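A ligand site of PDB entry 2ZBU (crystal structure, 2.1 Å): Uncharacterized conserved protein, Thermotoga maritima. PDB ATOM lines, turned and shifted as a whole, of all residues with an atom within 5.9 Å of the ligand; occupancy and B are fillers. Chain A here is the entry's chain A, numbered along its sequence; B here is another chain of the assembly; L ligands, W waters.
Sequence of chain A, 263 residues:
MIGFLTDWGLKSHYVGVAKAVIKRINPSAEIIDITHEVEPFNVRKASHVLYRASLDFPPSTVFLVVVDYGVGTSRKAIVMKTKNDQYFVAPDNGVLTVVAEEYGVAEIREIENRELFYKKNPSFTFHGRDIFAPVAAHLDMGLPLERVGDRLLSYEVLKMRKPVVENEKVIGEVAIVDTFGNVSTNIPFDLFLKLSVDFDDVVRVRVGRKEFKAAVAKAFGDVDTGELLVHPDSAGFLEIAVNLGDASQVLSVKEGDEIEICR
Water W1 lies within hydrogen-bond range of N of Gly 128 (2.9 Å), O1 of the ligand (2.9 Å), OD2 of Asp 68 (3.1 Å) and N of His 127 (3.1 Å).
The backbone NH of Asn 182 of chain B is in hydrogen-bond range of the side-chain carboxylate of Asp 178 of chain B, at 2.9 Å.
The backbone NH of Val 71 lies within hydrogen-bond range of the side-chain carboxylate of Asp 68 (3.5 Å).
The backbone NH (N) of Trp 8 is in hydrogen-bond range of the side-chain hydroxyl (OG1) of Thr 6, at 3.0 Å.
N of Phe 180 of chain B lies within hydrogen-bond range of OD1 of Asp 178 of chain B (3.0 Å).
O of Val 66 is in hydrogen-bond range of NE1 of Trp 8 (3.3 Å).
The backbone NH of Phe 41 lies within hydrogen-bond range of the side-chain carboxylate of Asp 7.
The backbone carbonyl oxygen of Phe 220 of chain B sits close to the side-chain amide nitrogen of Asn 243 of chain B (3.3 Å).
A nitrogen (N5) of the ligand lies close to the backbone carbonyl oxygen (O) of Tyr 69 (3.5 Å).
Residues that only touch the ligand: Phe 41 (3.5 Å), Val 67 (3.5 Å), Val 71 (3.9 Å), Phe 126 (3.5 Å), Phe 180 of chain B (3.5 Å), Phe 220 of chain B (3.4 Å), Asn 243 of chain B (3.6 Å) and Gly 245 of chain B (3.7 Å).
Hydrophobic or aromatic side chains within 4 Å of the ligand: Trp 8, Phe 41, Tyr 69, Val 71, Phe 126, Phe 180 of chain B and Phe 220 of chain B.
The nearest printed residue that does not touch the ligand is Ala 241 of chain B (4.1 Å).
O4 of the ligand is in hydrogen-bond range of OD2 of Asp 7 (2.7 Å).
The side-chain amide oxygen of Asn 182 of chain B lies within hydrogen-bond range of a nitrogen (N3) of the ligand (3.1 Å).
O of Val 66 is in hydrogen-bond range of O3 of the ligand (3.3 Å).
An oxygen (O3) of the ligand lies within hydrogen-bond range of the indole nitrogen (NE1) of Trp 8, 3.4 Å away.
The backbone carbonyl oxygen (O) of Val 242 of chain B sits at hydrogen-bond distance from a nitrogen (N3) of the ligand.
O3 of the ligand lies within hydrogen-bond range of N of Asp 68.
O1 of the ligand lies within hydrogen-bond range of O of Thr 125.
N of Leu 244 of chain B is in hydrogen-bond range of N4 of the ligand (2.8 Å).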
ATOM      1  N   THR A   6      19.599  24.908  31.226  1.00  0.00           N
ATOM      2  CA  THR A   6      20.089  24.746  29.858  1.00  0.00           C
ATOM      3  C   THR A   6      19.129  25.326  28.831  1.00  0.00           C
ATOM      4  O   THR A   6      18.032  25.787  29.170  1.00  0.00           O
ATOM      5  CB  THR A   6      20.249  23.239  29.462  1.00  0.00           C
ATOM      6  OG1 THR A   6      18.953  22.710  29.140  1.00  0.00           O
ATOM      7  CG2 THR A   6      20.860  22.428  30.599  1.00  0.00           C
ATOM      8  N   ASP A   7      19.549  25.257  27.576  1.00  0.00           N
ATOM      9  CA  ASP A   7      18.745  25.692  26.442  1.00  0.00           C
ATOM     10  C   ASP A   7      18.411  24.461  25.592  1.00  0.00           C
ATOM     11  O   ASP A   7      18.145  24.562  24.391  1.00  0.00           O
ATOM     12  CB  ASP A   7      19.545  26.700  25.608  1.00  0.00           C
ATOM     13  CG  ASP A   7      20.790  26.075  24.965  1.00  0.00           C
ATOM     14  OD1 ASP A   7      21.232  24.993  25.434  1.00  0.00           O
ATOM     15  OD2 ASP A   7      21.334  26.681  24.009  1.00  0.00           O
ATOM     16  N   TRP A   8      18.427  23.283  26.213  1.00  0.00           N
ATOM     17  CA  TRP A   8      18.182  22.038  25.491  1.00  0.00           C
ATOM     18  C   TRP A   8      16.722  21.687  25.226  1.00  0.00           C
ATOM     19  O   TRP A   8      16.419  20.907  24.314  1.00  0.00           O
ATOM     20  CB  TRP A   8      18.792  20.842  26.242  1.00  0.00           C
ATOM     21  CG  TRP A   8      20.225  20.995  26.660  1.00  0.00           C
ATOM     22  CD1 TRP A   8      21.119  21.959  26.285  1.00  0.00           C
ATOM     23  CD2 TRP A   8      20.933  20.123  27.555  1.00  0.00           C
ATOM     24  NE1 TRP A   8      22.328  21.757  26.896  1.00  0.00           N
ATOM     25  CE2 TRP A   8      22.250  20.641  27.685  1.00  0.00           C
ATOM     26  CE3 TRP A   8      20.580  18.969  28.278  1.00  0.00           C
ATOM     27  CZ2 TRP A   8      23.209  20.034  28.495  1.00  0.00           C
ATOM     28  CZ3 TRP A   8      21.540  18.375  29.083  1.00  0.00           C
ATOM     29  CH2 TRP A   8      22.839  18.910  29.194  1.00  0.00           C
ATOM     30  N   PRO A  40      17.525  29.051  22.502  1.00  0.00           N
ATOM     31  CA  PRO A  40      18.787  28.534  21.967  1.00  0.00           C
ATOM     32  C   PRO A  40      19.940  29.537  21.941  1.00  0.00           C
ATOM     33  O   PRO A  40      19.805  30.649  21.419  1.00  0.00           O
ATOM     34  CB  PRO A  40      18.389  28.055  20.581  1.00  0.00           C
ATOM     35  CG  PRO A  40      16.985  27.549  20.810  1.00  0.00           C
ATOM     36  CD  PRO A  40      16.395  28.681  21.628  1.00  0.00           C
ATOM     37  N   PHE A  41      21.056  29.136  22.546  1.00  0.00           N
ATOM     38  CA  PHE A  41      22.266  29.936  22.596  1.00  0.00           C
ATOM     39  C   PHE A  41      22.162  31.246  23.373  1.00  0.00           C
ATOM     40  O   PHE A  41      23.127  32.013  23.422  1.00  0.00           O
ATOM     41  CB  PHE A  41      22.750  30.290  21.172  1.00  0.00           C
ATOM     42  CG  PHE A  41      22.318  29.310  20.119  1.00  0.00           C
ATOM     43  CD1 PHE A  41      22.559  27.943  20.261  1.00  0.00           C
ATOM     44  CD2 PHE A  41      21.679  29.756  18.968  1.00  0.00           C
ATOM     45  CE1 PHE A  41      22.158  27.039  19.278  1.00  0.00           C
ATOM     46  CE2 PHE A  41      21.275  28.857  17.977  1.00  0.00           C
ATOM     47  CZ  PHE A  41      21.521  27.504  18.139  1.00  0.00           C
ATOM     48  N   VAL A  66      24.376  24.918  31.355  1.00  0.00           N
ATOM     49  CA  VAL A  66      24.856  24.599  30.032  1.00  0.00           C
ATOM     50  C   VAL A  66      24.074  25.184  28.855  1.00  0.00           C
ATOM     51  O   VAL A  66      23.148  24.556  28.336  1.00  0.00           O
ATOM     52  CB  VAL A  66      24.936  23.072  29.809  1.00  0.00           C
ATOM     53  CG1 VAL A  66      25.789  22.772  28.560  1.00  0.00           C
ATOM     54  CG2 VAL A  66      25.518  22.392  31.028  1.00  0.00           C
ATOM     55  N   VAL A  67      24.430  26.409  28.488  1.00  0.00           N
ATOM     56  CA  VAL A  67      23.891  27.076  27.305  1.00  0.00           C
ATOM     57  C   VAL A  67      25.275  27.271  26.680  1.00  0.00           C
ATOM     58  O   VAL A  67      25.996  28.210  26.992  1.00  0.00           O
ATOM     59  CB  VAL A  67      23.237  28.422  27.644  1.00  0.00           C
ATOM     60  CG1 VAL A  67      22.866  29.147  26.348  1.00  0.00           C
ATOM     61  CG2 VAL A  67      21.999  28.187  28.519  1.00  0.00           C
ATOM     62  N   ASP A  68      25.628  26.351  25.808  1.00  0.00           N
ATOM     63  CA  ASP A  68      26.988  26.325  25.295  1.00  0.00           C
ATOM     64  C   ASP A  68      27.159  26.169  23.771  1.00  0.00           C
ATOM     65  O   ASP A  68      27.561  25.119  23.273  1.00  0.00           O
ATOM     66  CB  ASP A  68      27.658  25.192  26.109  1.00  0.00           C
ATOM     67  CG  ASP A  68      29.114  24.989  25.797  1.00  0.00           C
ATOM     68  OD1 ASP A  68      29.822  25.965  25.510  1.00  0.00           O
ATOM     69  OD2 ASP A  68      29.539  23.824  25.895  1.00  0.00           O
ATOM     70  N   TYR A  69      26.875  27.244  23.053  1.00  0.00           N
ATOM     71  CA  TYR A  69      26.991  27.259  21.607  1.00  0.00           C
ATOM     72  C   TYR A  69      28.429  26.995  21.164  1.00  0.00           C
ATOM     73  O   TYR A  69      28.656  26.534  20.054  1.00  0.00           O
ATOM     74  CB  TYR A  69      26.489  28.601  21.048  1.00  0.00           C
ATOM     75  CG  TYR A  69      27.264  29.826  21.513  1.00  0.00           C
ATOM     76  CD1 TYR A  69      28.491  30.177  20.928  1.00  0.00           C
ATOM     77  CD2 TYR A  69      26.793  30.602  22.561  1.00  0.00           C
ATOM     78  CE1 TYR A  69      29.220  31.274  21.384  1.00  0.00           C
ATOM     79  CE2 TYR A  69      27.509  31.699  23.036  1.00  0.00           C
ATOM     80  CZ  TYR A  69      28.722  32.026  22.442  1.00  0.00           C
ATOM     81  OH  TYR A  69      29.428  33.100  22.931  1.00  0.00           O
ATOM     82  N   GLY A  70      29.386  27.294  22.032  1.00  0.00           N
ATOM     83  CA  GLY A  70      30.775  27.070  21.685  1.00  0.00           C
ATOM     84  C   GLY A  70      31.283  25.702  22.111  1.00  0.00           C
ATOM     85  O   GLY A  70      32.488  25.487  22.241  1.00  0.00           O
ATOM     86  N   VAL A  71      30.370  24.751  22.315  1.00  0.00           N
ATOM     87  CA  VAL A  71      30.786  23.411  22.737  1.00  0.00           C
ATOM     88  C   VAL A  71      31.804  22.807  21.767  1.00  0.00           C
ATOM     89  O   VAL A  71      31.668  22.927  20.547  1.00  0.00           O
ATOM     90  CB  VAL A  71      29.555  22.453  22.888  1.00  0.00           C
ATOM     91  CG1 VAL A  71      28.868  22.288  21.545  1.00  0.00           C
ATOM     92  CG2 VAL A  71      29.998  21.099  23.438  1.00  0.00           C
ATOM     93  N   THR A 125      30.148  17.680  20.653  1.00  0.00           N
ATOM     94  CA  THR A 125      29.056  18.633  20.829  1.00  0.00           C
ATOM     95  C   THR A 125      28.119  18.449  22.017  1.00  0.00           C
ATOM     96  O   THR A 125      27.068  19.094  22.085  1.00  0.00           O
ATOM     97  CB  THR A 125      28.210  18.718  19.535  1.00  0.00           C
ATOM     98  OG1 THR A 125      27.833  17.410  19.120  1.00  0.00           O
ATOM     99  CG2 THR A 125      29.022  19.396  18.404  1.00  0.00           C
ATOM    100  N   PHE A 126      28.466  17.581  22.960  1.00  0.00           N
ATOM    101  CA  PHE A 126      27.595  17.396  24.118  1.00  0.00           C
ATOM    102  C   PHE A 126      28.382  17.290  25.425  1.00  0.00           C
ATOM    103  O   PHE A 126      28.239  16.323  26.171  1.00  0.00           O
ATOM    104  CB  PHE A 126      26.697  16.162  23.927  1.00  0.00           C
ATOM    105  CG  PHE A 126      25.506  16.097  24.887  1.00  0.00           C
ATOM    106  CD1 PHE A 126      25.167  17.176  25.700  1.00  0.00           C
ATOM    107  CD2 PHE A 126      24.706  14.959  24.938  1.00  0.00           C
ATOM    108  CE1 PHE A 126      24.062  17.125  26.555  1.00  0.00           C
ATOM    109  CE2 PHE A 126      23.592  14.892  25.787  1.00  0.00           C
ATOM    110  CZ  PHE A 126      23.270  15.985  26.601  1.00  0.00           C
ATOM    111  N   HIS A 127      29.232  18.293  25.695  1.00  0.00           N
ATOM    112  CA  HIS A 127      30.017  18.302  26.923  1.00  0.00           C
ATOM    113  C   HIS A 127      29.079  18.376  28.133  1.00  0.00           C
ATOM    114  O   HIS A 127      29.451  18.021  29.243  1.00  0.00           O
ATOM    115  CB  HIS A 127      30.990  19.484  26.948  1.00  0.00           C
ATOM    116  CG  HIS A 127      32.100  19.381  25.947  1.00  0.00           C
ATOM    117  ND1 HIS A 127      32.253  18.277  25.124  1.00  0.00           N
ATOM    118  CD2 HIS A 127      33.129  20.214  25.657  1.00  0.00           C
ATOM    119  CE1 HIS A 127      33.336  18.448  24.366  1.00  0.00           C
ATOM    120  NE2 HIS A 127      33.881  19.605  24.676  1.00  0.00           N
ATOM    121  N   GLY A 128      27.842  18.837  27.906  1.00  0.00           N
ATOM    122  CA  GLY A 128      26.895  18.909  29.006  1.00  0.00           C
ATOM    123  C   GLY A 128      26.830  17.542  29.671  1.00  0.00           C
ATOM    124  O   GLY A 128      26.897  17.422  30.898  1.00  0.00           O
ATOM    125  N   ASP B 178      15.976  18.045  16.477  1.00  0.00           N
ATOM    126  CA  ASP B 178      15.885  18.510  17.857  1.00  0.00           C
ATOM    127  C   ASP B 178      15.457  19.980  17.947  1.00  0.00           C
ATOM    128  O   ASP B 178      15.197  20.610  16.932  1.00  0.00           O
ATOM    129  CB  ASP B 178      17.211  18.288  18.604  1.00  0.00           C
ATOM    130  CG  ASP B 178      18.345  19.178  18.103  1.00  0.00           C
ATOM    131  OD1 ASP B 178      18.106  20.109  17.315  1.00  0.00           O
ATOM    132  OD2 ASP B 178      19.494  18.933  18.527  1.00  0.00           O
ATOM    133  N   PHE B 180      17.059  22.669  18.411  1.00  0.00           N
ATOM    134  CA  PHE B 180      17.940  23.639  17.782  1.00  0.00           C
ATOM    135  C   PHE B 180      17.744  23.574  16.273  1.00  0.00           C
ATOM    136  O   PHE B 180      18.240  24.433  15.519  1.00  0.00           O
ATOM    137  CB  PHE B 180      19.405  23.316  18.106  1.00  0.00           C
ATOM    138  CG  PHE B 180      19.683  23.203  19.582  1.00  0.00           C
ATOM    139  CD1 PHE B 180      19.792  24.354  20.369  1.00  0.00           C
ATOM    140  CD2 PHE B 180      19.813  21.955  20.185  1.00  0.00           C
ATOM    141  CE1 PHE B 180      20.040  24.250  21.737  1.00  0.00           C
ATOM    142  CE2 PHE B 180      20.062  21.850  21.554  1.00  0.00           C
ATOM    143  CZ  PHE B 180      20.179  22.999  22.336  1.00  0.00           C
ATOM    144  N   ASN B 182      18.734  20.923  14.632  1.00  0.00           N
ATOM    145  CA  ASN B 182      19.767  19.994  14.158  1.00  0.00           C
ATOM    146  C   ASN B 182      19.058  18.814  13.504  1.00  0.00           C
ATOM    147  O   ASN B 182      18.005  18.377  13.961  1.00  0.00           O
ATOM    148  CB  ASN B 182      20.641  19.519  15.325  1.00  0.00           C
ATOM    149  CG  ASN B 182      21.407  20.647  15.998  1.00  0.00           C
ATOM    150  OD1 ASN B 182      21.880  21.570  15.330  1.00  0.00           O
ATOM    151  ND2 ASN B 182      21.533  20.590  17.324  1.00  0.00           N
ATOM    152  N   PHE B 220      30.182  22.770  16.325  1.00  0.00           N
ATOM    153  CA  PHE B 220      29.405  23.735  15.543  1.00  0.00           C
ATOM    154  C   PHE B 220      30.278  24.954  15.259  1.00  0.00           C
ATOM    155  O   PHE B 220      30.305  25.485  14.145  1.00  0.00           O
ATOM    156  CB  PHE B 220      28.172  24.191  16.328  1.00  0.00           C
ATOM    157  CG  PHE B 220      27.338  23.061  16.862  1.00  0.00           C
ATOM    158  CD1 PHE B 220      26.582  22.262  16.000  1.00  0.00           C
ATOM    159  CD2 PHE B 220      27.293  22.807  18.231  1.00  0.00           C
ATOM    160  CE1 PHE B 220      25.797  21.224  16.507  1.00  0.00           C
ATOM    161  CE2 PHE B 220      26.516  21.772  18.749  1.00  0.00           C
ATOM    162  CZ  PHE B 220      25.773  20.979  17.884  1.00  0.00           C
ATOM    163  N   GLY B 221      30.997  25.373  16.292  1.00  0.00           N
ATOM    164  CA  GLY B 221      31.866  26.530  16.185  1.00  0.00           C
ATOM    165  C   GLY B 221      33.016  26.382  15.212  1.00  0.00           C
ATOM    166  O   GLY B 221      33.743  27.352  14.977  1.00  0.00           O
ATOM    167  N   ALA B 241      23.946  20.243  10.873  1.00  0.00           N
ATOM    168  CA  ALA B 241      23.536  21.399  11.652  1.00  0.00           C
ATOM    169  C   ALA B 241      24.008  22.705  11.021  1.00  0.00           C
ATOM    170  O   ALA B 241      24.855  22.724  10.122  1.00  0.00           O
ATOM    171  CB  ALA B 241      24.098  21.299  13.086  1.00  0.00           C
ATOM    172  N   VAL B 242      23.425  23.790  11.506  1.00  0.00           N
ATOM    173  CA  VAL B 242      23.779  25.128  11.097  1.00  0.00           C
ATOM    174  C   VAL B 242      24.357  25.727  12.378  1.00  0.00           C
ATOM    175  O   VAL B 242      23.697  25.731  13.422  1.00  0.00           O
ATOM    176  CB  VAL B 242      22.541  25.940  10.673  1.00  0.00           C
ATOM    177  CG1 VAL B 242      22.893  27.411  10.560  1.00  0.00           C
ATOM    178  CG2 VAL B 242      22.017  25.429   9.335  1.00  0.00           C
ATOM    179  N   ASN B 243      25.597  26.188  12.318  1.00  0.00           N
ATOM    180  CA  ASN B 243      26.204  26.757  13.506  1.00  0.00           C
ATOM    181  C   ASN B 243      25.416  27.985  13.944  1.00  0.00           C
ATOM    182  O   ASN B 243      25.339  28.981  13.224  1.00  0.00           O
ATOM    183  CB  ASN B 243      27.673  27.116  13.220  1.00  0.00           C
ATOM    184  CG  ASN B 243      28.339  27.812  14.397  1.00  0.00           C
ATOM    185  OD1 ASN B 243      27.965  27.581  15.547  1.00  0.00           O
ATOM    186  ND2 ASN B 243      29.336  28.650  14.112  1.00  0.00           N
ATOM    187  N   LEU B 244      24.793  27.884  15.120  1.00  0.00           N
ATOM    188  CA  LEU B 244      23.989  28.983  15.636  1.00  0.00           C
ATOM    189  C   LEU B 244      22.784  29.236  14.753  1.00  0.00           C
ATOM    190  O   LEU B 244      22.311  30.361  14.638  1.00  0.00           O
ATOM    191  CB  LEU B 244      24.830  30.250  15.758  1.00  0.00           C
ATOM    192  CG  LEU B 244      25.858  30.185  16.885  1.00  0.00           C
ATOM    193  CD1 LEU B 244      26.951  31.241  16.680  1.00  0.00           C
ATOM    194  CD2 LEU B 244      25.127  30.392  18.236  1.00  0.00           C
ATOM    195  N   GLY B 245      22.287  28.169  14.126  1.00  0.00           N
ATOM    196  CA  GLY B 245      21.136  28.270  13.251  1.00  0.00           C
ATOM    197  C   GLY B 245      20.319  26.998  13.265  1.00  0.00           C
ATOM    198  O   GLY B 245      20.633  26.057  14.002  1.00  0.00           O
HETATM  199  O1  LIG L   1      26.094  20.564  24.096  1.00  0.00           O
HETATM  200  C1  LIG L   1      24.894  21.272  24.381  1.00  0.00           C
HETATM  201  C2  LIG L   1      24.974  22.640  23.721  1.00  0.00           C
HETATM  202  O2  LIG L   1      25.087  22.558  22.280  1.00  0.00           O
HETATM  203  C3  LIG L   1      23.720  23.500  23.999  1.00  0.00           C
HETATM  204  O3  LIG L   1      23.907  24.256  25.185  1.00  0.00           O
HETATM  205  C4  LIG L   1      23.579  24.345  22.714  1.00  0.00           C
HETATM  206  O4  LIG L   1      23.697  25.750  23.000  1.00  0.00           O
HETATM  207  C5  LIG L   1      24.691  23.857  21.774  1.00  0.00           C
HETATM  208  N1  LIG L   1      24.190  23.749  20.386  1.00  0.00           N
HETATM  209  C6  LIG L   1      23.228  22.877  19.932  1.00  0.00           C
HETATM  210  N2  LIG L   1      23.019  23.049  18.650  1.00  0.00           N
HETATM  211  C7  LIG L   1      23.832  24.048  18.207  1.00  0.00           C
HETATM  212  C8  LIG L   1      24.063  24.679  16.939  1.00  0.00           C
HETATM  213  N3  LIG L   1      23.360  24.281  15.824  1.00  0.00           N
HETATM  214  N4  LIG L   1      24.971  25.669  16.863  1.00  0.00           N
HETATM  215  C9  LIG L   1      25.666  26.071  17.946  1.00  0.00           C
HETATM  216  N5  LIG L   1      25.488  25.509  19.145  1.00  0.00           N
HETATM  217  C10 LIG L   1      24.592  24.509  19.323  1.00  0.00           C
HETATM  218  O   HOH W   1      28.040  21.159  26.216  1.00  0.00           O
